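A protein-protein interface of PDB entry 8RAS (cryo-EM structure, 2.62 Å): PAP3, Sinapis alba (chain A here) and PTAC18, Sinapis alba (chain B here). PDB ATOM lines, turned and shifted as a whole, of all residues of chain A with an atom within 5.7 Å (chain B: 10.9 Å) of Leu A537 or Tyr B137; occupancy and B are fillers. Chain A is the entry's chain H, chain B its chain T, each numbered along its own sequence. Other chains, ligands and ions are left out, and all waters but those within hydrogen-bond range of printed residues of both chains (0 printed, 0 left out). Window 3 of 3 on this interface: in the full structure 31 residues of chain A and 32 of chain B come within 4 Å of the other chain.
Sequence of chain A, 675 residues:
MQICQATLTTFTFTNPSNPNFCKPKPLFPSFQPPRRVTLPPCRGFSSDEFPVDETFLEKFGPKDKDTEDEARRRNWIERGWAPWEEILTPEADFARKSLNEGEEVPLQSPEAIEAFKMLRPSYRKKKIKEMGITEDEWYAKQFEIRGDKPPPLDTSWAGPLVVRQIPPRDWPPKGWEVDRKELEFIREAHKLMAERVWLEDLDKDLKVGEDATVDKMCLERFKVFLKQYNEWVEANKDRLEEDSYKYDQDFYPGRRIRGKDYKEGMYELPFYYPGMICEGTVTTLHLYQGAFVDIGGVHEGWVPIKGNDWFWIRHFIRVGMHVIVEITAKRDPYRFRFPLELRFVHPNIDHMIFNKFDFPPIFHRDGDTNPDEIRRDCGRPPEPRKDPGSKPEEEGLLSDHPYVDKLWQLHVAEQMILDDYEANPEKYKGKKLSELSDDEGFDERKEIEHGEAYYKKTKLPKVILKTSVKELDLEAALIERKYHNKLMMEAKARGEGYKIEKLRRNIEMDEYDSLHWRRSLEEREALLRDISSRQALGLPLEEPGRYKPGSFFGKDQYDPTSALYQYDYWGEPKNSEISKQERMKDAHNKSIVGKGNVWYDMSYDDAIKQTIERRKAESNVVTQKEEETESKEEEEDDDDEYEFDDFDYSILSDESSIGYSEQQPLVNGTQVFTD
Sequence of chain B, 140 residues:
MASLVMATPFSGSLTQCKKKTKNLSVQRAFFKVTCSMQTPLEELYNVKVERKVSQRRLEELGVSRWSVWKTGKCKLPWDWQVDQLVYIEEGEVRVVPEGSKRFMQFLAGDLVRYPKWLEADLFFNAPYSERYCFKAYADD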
ATOM      1  N   ARG A 529     -25.749  12.124 -25.690  1.00  0.00           N
ATOM      2  CA  ARG A 529     -24.844  13.107 -25.103  1.00  0.00           C
ATOM      3  C   ARG A 529     -23.389  12.768 -25.407  1.00  0.00           C
ATOM      4  O   ARG A 529     -22.572  13.671 -25.634  1.00  0.00           O
ATOM      5  CB  ARG A 529     -25.072  13.210 -23.596  1.00  0.00           C
ATOM      6  CG  ARG A 529     -26.478  13.644 -23.217  1.00  0.00           C
ATOM      7  CD  ARG A 529     -26.547  14.130 -21.777  1.00  0.00           C
ATOM      8  NE  ARG A 529     -26.822  13.055 -20.832  1.00  0.00           N
ATOM      9  CZ  ARG A 529     -26.052  12.755 -19.795  1.00  0.00           C
ATOM     10  NH1 ARG A 529     -24.946  13.435 -19.537  1.00  0.00           N
ATOM     11  NH2 ARG A 529     -26.401  11.753 -18.994  1.00  0.00           N
ATOM     12  N   ASP A 530     -23.052  11.475 -25.427  1.00  0.00           N
ATOM     13  CA  ASP A 530     -21.697  11.060 -25.774  1.00  0.00           C
ATOM     14  C   ASP A 530     -21.351  11.437 -27.212  1.00  0.00           C
ATOM     15  O   ASP A 530     -20.252  11.930 -27.483  1.00  0.00           O
ATOM     16  CB  ASP A 530     -21.539   9.553 -25.564  1.00  0.00           C
ATOM     17  CG  ASP A 530     -21.113   9.205 -24.154  1.00  0.00           C
ATOM     18  OD1 ASP A 530     -20.031   9.661 -23.726  1.00  0.00           O
ATOM     19  OD2 ASP A 530     -21.861   8.473 -23.476  1.00  0.00           O
ATOM     20  N   SER A 532     -22.693  13.885 -28.934  1.00  0.00           N
ATOM     21  CA  SER A 532     -22.556  15.339 -28.962  1.00  0.00           C
ATOM     22  C   SER A 532     -21.174  15.763 -28.482  1.00  0.00           C
ATOM     23  O   SER A 532     -20.455  16.490 -29.181  1.00  0.00           O
ATOM     24  CB  SER A 532     -23.645  15.984 -28.105  1.00  0.00           C
ATOM     25  OG  SER A 532     -23.239  16.071 -26.751  1.00  0.00           O
ATOM     26  N   SER A 533     -20.765  15.273 -27.309  1.00  0.00           N
ATOM     27  CA  SER A 533     -19.475  15.666 -26.749  1.00  0.00           C
ATOM     28  C   SER A 533     -18.316  15.226 -27.638  1.00  0.00           C
ATOM     29  O   SER A 533     -17.377  15.997 -27.871  1.00  0.00           O
ATOM     30  CB  SER A 533     -19.322  15.088 -25.343  1.00  0.00           C
ATOM     31  OG  SER A 533     -20.437  15.419 -24.534  1.00  0.00           O
ATOM     32  N   ARG A 534     -18.366  13.994 -28.152  1.00  0.00           N
ATOM     33  CA  ARG A 534     -17.235  13.458 -28.902  1.00  0.00           C
ATOM     34  C   ARG A 534     -17.071  14.157 -30.247  1.00  0.00           C
ATOM     35  O   ARG A 534     -15.959  14.547 -30.618  1.00  0.00           O
ATOM     36  CB  ARG A 534     -17.393  11.947 -29.080  1.00  0.00           C
ATOM     37  CG  ARG A 534     -17.186  11.165 -27.790  1.00  0.00           C
ATOM     38  CD  ARG A 534     -17.491   9.687 -27.964  1.00  0.00           C
ATOM     39  NE  ARG A 534     -17.340   8.950 -26.715  1.00  0.00           N
ATOM     40  CZ  ARG A 534     -16.175   8.618 -26.174  1.00  0.00           C
ATOM     41  NH1 ARG A 534     -15.028   8.945 -26.746  1.00  0.00           N
ATOM     42  NH2 ARG A 534     -16.160   7.940 -25.030  1.00  0.00           N
ATOM     43  N   GLN A 535     -18.163  14.327 -30.998  1.00  0.00           N
ATOM     44  CA  GLN A 535     -18.073  15.097 -32.232  1.00  0.00           C
ATOM     45  C   GLN A 535     -17.783  16.570 -31.984  1.00  0.00           C
ATOM     46  O   GLN A 535     -17.297  17.251 -32.892  1.00  0.00           O
ATOM     47  CB  GLN A 535     -19.349  14.938 -33.056  1.00  0.00           C
ATOM     48  CG  GLN A 535     -19.249  13.877 -34.141  1.00  0.00           C
ATOM     49  CD  GLN A 535     -19.978  12.607 -33.786  1.00  0.00           C
ATOM     50  OE1 GLN A 535     -20.150  12.292 -32.613  1.00  0.00           O
ATOM     51  NE2 GLN A 535     -20.430  11.878 -34.799  1.00  0.00           N
ATOM     52  N   ALA A 536     -18.065  17.082 -30.784  1.00  0.00           N
ATOM     53  CA  ALA A 536     -17.600  18.422 -30.458  1.00  0.00           C
ATOM     54  C   ALA A 536     -16.107  18.448 -30.155  1.00  0.00           C
ATOM     55  O   ALA A 536     -15.463  19.488 -30.326  1.00  0.00           O
ATOM     56  CB  ALA A 536     -18.386  18.979 -29.273  1.00  0.00           C
ATOM     57  N   LEU A 537     -15.543  17.324 -29.709  1.00  0.00           N
ATOM     58  CA  LEU A 537     -14.145  17.276 -29.306  1.00  0.00           C
ATOM     59  C   LEU A 537     -13.297  16.305 -30.118  1.00  0.00           C
ATOM     60  O   LEU A 537     -12.109  16.146 -29.817  1.00  0.00           O
ATOM     61  CB  LEU A 537     -14.043  16.922 -27.817  1.00  0.00           C
ATOM     62  CG  LEU A 537     -14.631  17.986 -26.889  1.00  0.00           C
ATOM     63  CD1 LEU A 537     -14.948  17.399 -25.528  1.00  0.00           C
ATOM     64  CD2 LEU A 537     -13.687  19.169 -26.762  1.00  0.00           C
ATOM     65  N   GLY A 538     -13.861  15.650 -31.131  1.00  0.00           N
ATOM     66  CA  GLY A 538     -13.079  14.804 -32.008  1.00  0.00           C
ATOM     67  C   GLY A 538     -12.709  13.446 -31.458  1.00  0.00           C
ATOM     68  O   GLY A 538     -11.925  12.733 -32.095  1.00  0.00           O
ATOM     69  N   LEU A 539     -13.240  13.060 -30.301  1.00  0.00           N
ATOM     70  CA  LEU A 539     -12.937  11.752 -29.746  1.00  0.00           C
ATOM     71  C   LEU A 539     -13.573  10.652 -30.598  1.00  0.00           C
ATOM     72  O   LEU A 539     -14.593  10.875 -31.255  1.00  0.00           O
ATOM     73  CB  LEU A 539     -13.439  11.653 -28.309  1.00  0.00           C
ATOM     74  CG  LEU A 539     -12.516  12.215 -27.228  1.00  0.00           C
ATOM     75  CD1 LEU A 539     -13.288  12.440 -25.943  1.00  0.00           C
ATOM     76  CD2 LEU A 539     -11.339  11.287 -26.989  1.00  0.00           C
ATOM     77  N   GLN B  81     -21.702   0.405 -24.458  1.00  0.00           N
ATOM     78  CA  GLN B  81     -21.239   1.505 -25.290  1.00  0.00           C
ATOM     79  C   GLN B  81     -21.365   2.852 -24.592  1.00  0.00           C
ATOM     80  O   GLN B  81     -21.070   3.883 -25.205  1.00  0.00           O
ATOM     81  CB  GLN B  81     -21.988   1.503 -26.625  1.00  0.00           C
ATOM     82  CG  GLN B  81     -23.493   1.576 -26.506  1.00  0.00           C
ATOM     83  CD  GLN B  81     -24.192   0.773 -27.590  1.00  0.00           C
ATOM     84  OE1 GLN B  81     -23.656  -0.217 -28.084  1.00  0.00           O
ATOM     85  NE2 GLN B  81     -25.392   1.200 -27.963  1.00  0.00           N
ATOM     86  N   VAL B  82     -21.804   2.863 -23.333  1.00  0.00           N
ATOM     87  CA  VAL B  82     -21.765   4.036 -22.471  1.00  0.00           C
ATOM     88  C   VAL B  82     -21.234   3.603 -21.111  1.00  0.00           C
ATOM     89  O   VAL B  82     -21.429   2.460 -20.685  1.00  0.00           O
ATOM     90  CB  VAL B  82     -23.153   4.706 -22.321  1.00  0.00           C
ATOM     91  CG1 VAL B  82     -23.019   6.078 -21.686  1.00  0.00           C
ATOM     92  CG2 VAL B  82     -23.861   4.810 -23.665  1.00  0.00           C
ATOM     93  N   ASP B  83     -20.549   4.519 -20.429  1.00  0.00           N
ATOM     94  CA  ASP B  83     -20.112   4.264 -19.064  1.00  0.00           C
ATOM     95  C   ASP B  83     -21.313   4.186 -18.126  1.00  0.00           C
ATOM     96  O   ASP B  83     -22.349   4.816 -18.353  1.00  0.00           O
ATOM     97  CB  ASP B  83     -19.155   5.357 -18.590  1.00  0.00           C
ATOM     98  CG  ASP B  83     -17.765   5.209 -19.175  1.00  0.00           C
ATOM     99  OD1 ASP B  83     -17.333   4.060 -19.402  1.00  0.00           O
ATOM    100  OD2 ASP B  83     -17.102   6.243 -19.402  1.00  0.00           O
ATOM    101  N   GLN B  84     -21.166   3.403 -17.058  1.00  0.00           N
ATOM    102  CA  GLN B  84     -22.263   3.211 -16.112  1.00  0.00           C
ATOM    103  C   GLN B  84     -21.714   2.704 -14.789  1.00  0.00           C
ATOM    104  O   GLN B  84     -21.141   1.611 -14.739  1.00  0.00           O
ATOM    105  CB  GLN B  84     -23.291   2.227 -16.670  1.00  0.00           C
ATOM    106  CG  GLN B  84     -24.314   1.754 -15.650  1.00  0.00           C
ATOM    107  CD  GLN B  84     -24.743   0.318 -15.877  1.00  0.00           C
ATOM    108  OE1 GLN B  84     -23.923  -0.599 -15.848  1.00  0.00           O
ATOM    109  NE2 GLN B  84     -26.035   0.114 -16.101  1.00  0.00           N
ATOM    110  N   LEU B  85     -21.889   3.485 -13.726  1.00  0.00           N
ATOM    111  CA  LEU B  85     -21.634   2.983 -12.385  1.00  0.00           C
ATOM    112  C   LEU B  85     -22.838   2.191 -11.892  1.00  0.00           C
ATOM    113  O   LEU B  85     -23.981   2.462 -12.266  1.00  0.00           O
ATOM    114  CB  LEU B  85     -21.331   4.117 -11.403  1.00  0.00           C
ATOM    115  CG  LEU B  85     -20.432   5.285 -11.810  1.00  0.00           C
ATOM    116  CD1 LEU B  85     -21.229   6.370 -12.503  1.00  0.00           C
ATOM    117  CD2 LEU B  85     -19.709   5.845 -10.597  1.00  0.00           C
ATOM    118  N   ARG B 113     -17.975   0.598 -11.805  1.00  0.00           N
ATOM    119  CA  ARG B 113     -18.154   1.435 -12.987  1.00  0.00           C
ATOM    120  C   ARG B 113     -17.787   0.615 -14.218  1.00  0.00           C
ATOM    121  O   ARG B 113     -16.606   0.342 -14.457  1.00  0.00           O
ATOM    122  CB  ARG B 113     -17.302   2.699 -12.894  1.00  0.00           C
ATOM    123  CG  ARG B 113     -17.421   3.616 -14.096  1.00  0.00           C
ATOM    124  CD  ARG B 113     -16.462   4.788 -13.986  1.00  0.00           C
ATOM    125  NE  ARG B 113     -16.562   5.687 -15.128  1.00  0.00           N
ATOM    126  CZ  ARG B 113     -17.083   6.905 -15.079  1.00  0.00           C
ATOM    127  NH1 ARG B 113     -17.565   7.406 -13.954  1.00  0.00           N
ATOM    128  NH2 ARG B 113     -17.122   7.639 -16.187  1.00  0.00           N
ATOM    129  N   LYS B 116     -16.854   1.882 -21.051  1.00  0.00           N
ATOM    130  CA  LYS B 116     -17.406   1.934 -22.395  1.00  0.00           C
ATOM    131  C   LYS B 116     -16.735   0.890 -23.285  1.00  0.00           C
ATOM    132  O   LYS B 116     -15.560   0.556 -23.110  1.00  0.00           O
ATOM    133  CB  LYS B 116     -17.227   3.336 -22.982  1.00  0.00           C
ATOM    134  CG  LYS B 116     -17.811   3.534 -24.370  1.00  0.00           C
ATOM    135  CD  LYS B 116     -17.801   5.003 -24.756  1.00  0.00           C
ATOM    136  CE  LYS B 116     -18.086   5.196 -26.235  1.00  0.00           C
ATOM    137  NZ  LYS B 116     -19.475   4.805 -26.599  1.00  0.00           N
ATOM    138  N   TRP B 117     -17.511   0.359 -24.231  1.00  0.00           N
ATOM    139  CA  TRP B 117     -17.107  -0.654 -25.207  1.00  0.00           C
ATOM    140  C   TRP B 117     -16.869  -2.023 -24.584  1.00  0.00           C
ATOM    141  O   TRP B 117     -16.349  -2.918 -25.261  1.00  0.00           O
ATOM    142  CB  TRP B 117     -15.858  -0.236 -25.990  1.00  0.00           C
ATOM    143  CG  TRP B 117     -16.049   0.989 -26.816  1.00  0.00           C
ATOM    144  CD1 TRP B 117     -17.077   1.249 -27.672  1.00  0.00           C
ATOM    145  CD2 TRP B 117     -15.186   2.130 -26.865  1.00  0.00           C
ATOM    146  NE1 TRP B 117     -16.908   2.481 -28.253  1.00  0.00           N
ATOM    147  CE2 TRP B 117     -15.754   3.043 -27.774  1.00  0.00           C
ATOM    148  CE3 TRP B 117     -13.989   2.468 -26.228  1.00  0.00           C
ATOM    149  CZ2 TRP B 117     -15.165   4.270 -28.063  1.00  0.00           C
ATOM    150  CZ3 TRP B 117     -13.408   3.684 -26.516  1.00  0.00           C
ATOM    151  CH2 TRP B 117     -13.994   4.572 -27.425  1.00  0.00           C
ATOM    152  N   CYS B 133     -25.911   4.757 -12.679  1.00  0.00           N
ATOM    153  CA  CYS B 133     -25.903   6.093 -13.265  1.00  0.00           C
ATOM    154  C   CYS B 133     -25.152   6.028 -14.587  1.00  0.00           C
ATOM    155  O   CYS B 133     -23.919   5.969 -14.590  1.00  0.00           O
ATOM    156  CB  CYS B 133     -25.274   7.107 -12.318  1.00  0.00           C
ATOM    157  SG  CYS B 133     -26.060   8.738 -12.383  1.00  0.00           S
ATOM    158  N   PHE B 134     -25.890   6.052 -15.696  1.00  0.00           N
ATOM    159  CA  PHE B 134     -25.256   6.140 -17.005  1.00  0.00           C
ATOM    160  C   PHE B 134     -24.646   7.523 -17.173  1.00  0.00           C
ATOM    161  O   PHE B 134     -25.325   8.538 -16.988  1.00  0.00           O
ATOM    162  CB  PHE B 134     -26.267   5.864 -18.120  1.00  0.00           C
ATOM    163  CG  PHE B 134     -26.639   4.414 -18.260  1.00  0.00           C
ATOM    164  CD1 PHE B 134     -25.726   3.496 -18.742  1.00  0.00           C
ATOM    165  CD2 PHE B 134     -27.898   3.971 -17.897  1.00  0.00           C
ATOM    166  CE1 PHE B 134     -26.060   2.165 -18.867  1.00  0.00           C
ATOM    167  CE2 PHE B 134     -28.240   2.637 -18.019  1.00  0.00           C
ATOM    168  CZ  PHE B 134     -27.319   1.734 -18.506  1.00  0.00           C
ATOM    169  N   LYS B 135     -23.361   7.564 -17.508  1.00  0.00           N
ATOM    170  CA  LYS B 135     -22.611   8.807 -17.588  1.00  0.00           C
ATOM    171  C   LYS B 135     -22.018   8.940 -18.981  1.00  0.00           C
ATOM    172  O   LYS B 135     -21.451   7.980 -19.513  1.00  0.00           O
ATOM    173  CB  LYS B 135     -21.504   8.849 -16.530  1.00  0.00           C
ATOM    174  CG  LYS B 135     -21.995   8.544 -15.126  1.00  0.00           C
ATOM    175  CD  LYS B 135     -22.621   9.754 -14.451  1.00  0.00           C
ATOM    176  CE  LYS B 135     -21.872  11.030 -14.784  1.00  0.00           C
ATOM    177  NZ  LYS B 135     -22.748  12.227 -14.683  1.00  0.00           N
ATOM    178  N   ALA B 136     -22.163  10.122 -19.569  1.00  0.00           N
ATOM    179  CA  ALA B 136     -21.570  10.416 -20.864  1.00  0.00           C
ATOM    180  C   ALA B 136     -20.128  10.873 -20.654  1.00  0.00           C
ATOM    181  O   ALA B 136     -19.552  10.712 -19.575  1.00  0.00           O
ATOM    182  CB  ALA B 136     -22.406  11.452 -21.609  1.00  0.00           C
ATOM    183  N   TYR B 137     -19.526  11.442 -21.694  1.00  0.00           N
ATOM    184  CA  TYR B 137     -18.172  11.959 -21.573  1.00  0.00           C
ATOM    185  C   TYR B 137     -18.139  13.100 -20.561  1.00  0.00           C
ATOM    186  O   TYR B 137     -19.114  13.834 -20.388  1.00  0.00           O
ATOM    187  CB  TYR B 137     -17.661  12.443 -22.930  1.00  0.00           C
ATOM    188  CG  TYR B 137     -16.248  12.979 -22.891  1.00  0.00           C
ATOM    189  CD1 TYR B 137     -15.909  14.145 -23.560  1.00  0.00           C
ATOM    190  CD2 TYR B 137     -15.247  12.300 -22.207  1.00  0.00           C
ATOM    191  CE1 TYR B 137     -14.619  14.635 -23.524  1.00  0.00           C
ATOM    192  CE2 TYR B 137     -13.955  12.783 -22.169  1.00  0.00           C
ATOM    193  CZ  TYR B 137     -13.646  13.950 -22.831  1.00  0.00           C
ATOM    194  OH  TYR B 137     -12.359  14.436 -22.802  1.00  0.00           O
ATOM    195  N   ALA B 138     -16.998  13.229 -19.878  1.00  0.00           N
ATOM    196  CA  ALA B 138     -16.806  14.213 -18.819  1.00  0.00           C
ATOM    197  C   ALA B 138     -17.809  13.984 -17.697  1.00  0.00           C
ATOM    198  O   ALA B 138     -17.761  12.948 -17.023  1.00  0.00           O
ATOM    199  CB  ALA B 138     -16.913  15.641 -19.363  1.00  0.00           C
ATOM    200  N   ASP B 139     -18.714  14.942 -17.490  1.00  0.00           N
ATOM    201  CA  ASP B 139     -19.761  14.827 -16.481  1.00  0.00           C
ATOM    202  C   ASP B 139     -19.165  14.591 -15.099  1.00  0.00           C
ATOM    203  O   ASP B 139     -18.789  15.542 -14.406  1.00  0.00           O
ATOM    204  CB  ASP B 139     -20.737  13.705 -16.845  1.00  0.00           C
ATOM    205  CG  ASP B 139     -21.458  13.959 -18.153  1.00  0.00           C
ATOM    206  OD1 ASP B 139     -21.156  14.976 -18.812  1.00  0.00           O
ATOM    207  OD2 ASP B 139     -22.327  13.142 -18.523  1.00  0.00           O
ATOM    208  N   ASP B 140     -19.080  13.330 -14.690  1.00  0.00           N
ATOM    209  CA  ASP B 140     -18.489  12.979 -13.403  1.00  0.00           C
ATOM    210  C   ASP B 140     -17.484  11.843 -13.556  1.00  0.00           C
ATOM    211  O   ASP B 140     -17.863  10.689 -13.761  1.00  0.00           O
ATOM    212  CB  ASP B 140     -19.577  12.588 -12.401  1.00  0.00           C
ATOM    213  CG  ASP B 140     -20.534  13.725 -12.106  1.00  0.00           C
ATOM    214  OD2 ASP B 140     -21.200  13.682 -11.050  1.00  0.00           O
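N of Tyr B137 sits at hydrogen-bond distance from OD1 of Asp A530.
OD2 of Asp B139 is in salt-bridge range of NH1 of Arg A529, 2.8 Å away.
The side-chain carboxylate of Asp B83 lies within hydrogen-bond range of the backbone NH of Lys B116 (2.8 Å).
The side-chain amino group (NZ) of Lys B135 is in salt-bridge range of the side-chain carboxylate (OD2) of Asp B139, at 3.97 Å.
OD2 of Asp B139 sits at hydrogen-bond distance from N of Ala B136.
O of Arg A529 is in hydrogen-bond range of OG of Ser A532.
The backbone carbonyl oxygen (O) of Arg A529 sits at hydrogen-bond distance from the side-chain hydroxyl (OG) of Ser A533 (3.0 Å).
The backbone carbonyl oxygen of Arg A534 sits at hydrogen-bond distance from the backbone NH of Leu A539, at 3.1 Å.
Phe B134 touches Arg A529 (O to NH2, 3.9 Å).
Ala B136 touches Arg A529 (CB to CB, 3.8 Å).
Val B82 touches Asp A530 (CG1 to OD2, 3.2 Å).
Asp A530 touches Ala B136.
CB of Ser A533 touches CB of Tyr B137, 3.9 Å away.
Arg A534 touches Lys B116.
Tyr B137 touches Leu A537 (CE1 to CD1, 3.4 Å).
Leu A539 touches Tyr B137.
Leu A537 touches just one residue of chain B: Tyr B137 (3.4 Å).
Tyr B137 touches just these residues of chain A: Asp A530 (2.7 Å), Ser A533 (3.9 Å), Leu A537 (3.4 Å) and Leu A539 (3.5 Å).
Of the printed residues of chain B, Ser A533 touches Tyr B137 (3.9 Å).
No residue of chain B comes within 4 Å of Gly A538.
Of the printed residues of chain A, Phe B134 touches Arg A529 (3.9 Å).
Of the printed residues of chain A, Lys B116 touches Arg A534 (3.4 Å).
Cys B133 touches none of the printed residues of chain A.
The nearest printed residue of chain A that does not touch Lys B116 is Asp A530 (5.3 Å).
Of the 16 printed residues of chain B, 6 touch a printed residue of chain A.
Along chain B the printed residues that touch a printed residue of chain A span positions 82 to 139.
Hydrophobic or aromatic side chains of chain A within 4 Å of the printed part of chain B: Leu A537 and Leu A539.
Along chain A the printed residues that touch a printed residue of chain B span positions 529 to 539.
Among the printed residues, 10 pairs touch across the chains.
Among the printed residues, Asp or Glu carboxylates within 4 Å of a Lys or Arg side-chain nitrogen of the other chain: Arg A529 with Asp B139.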
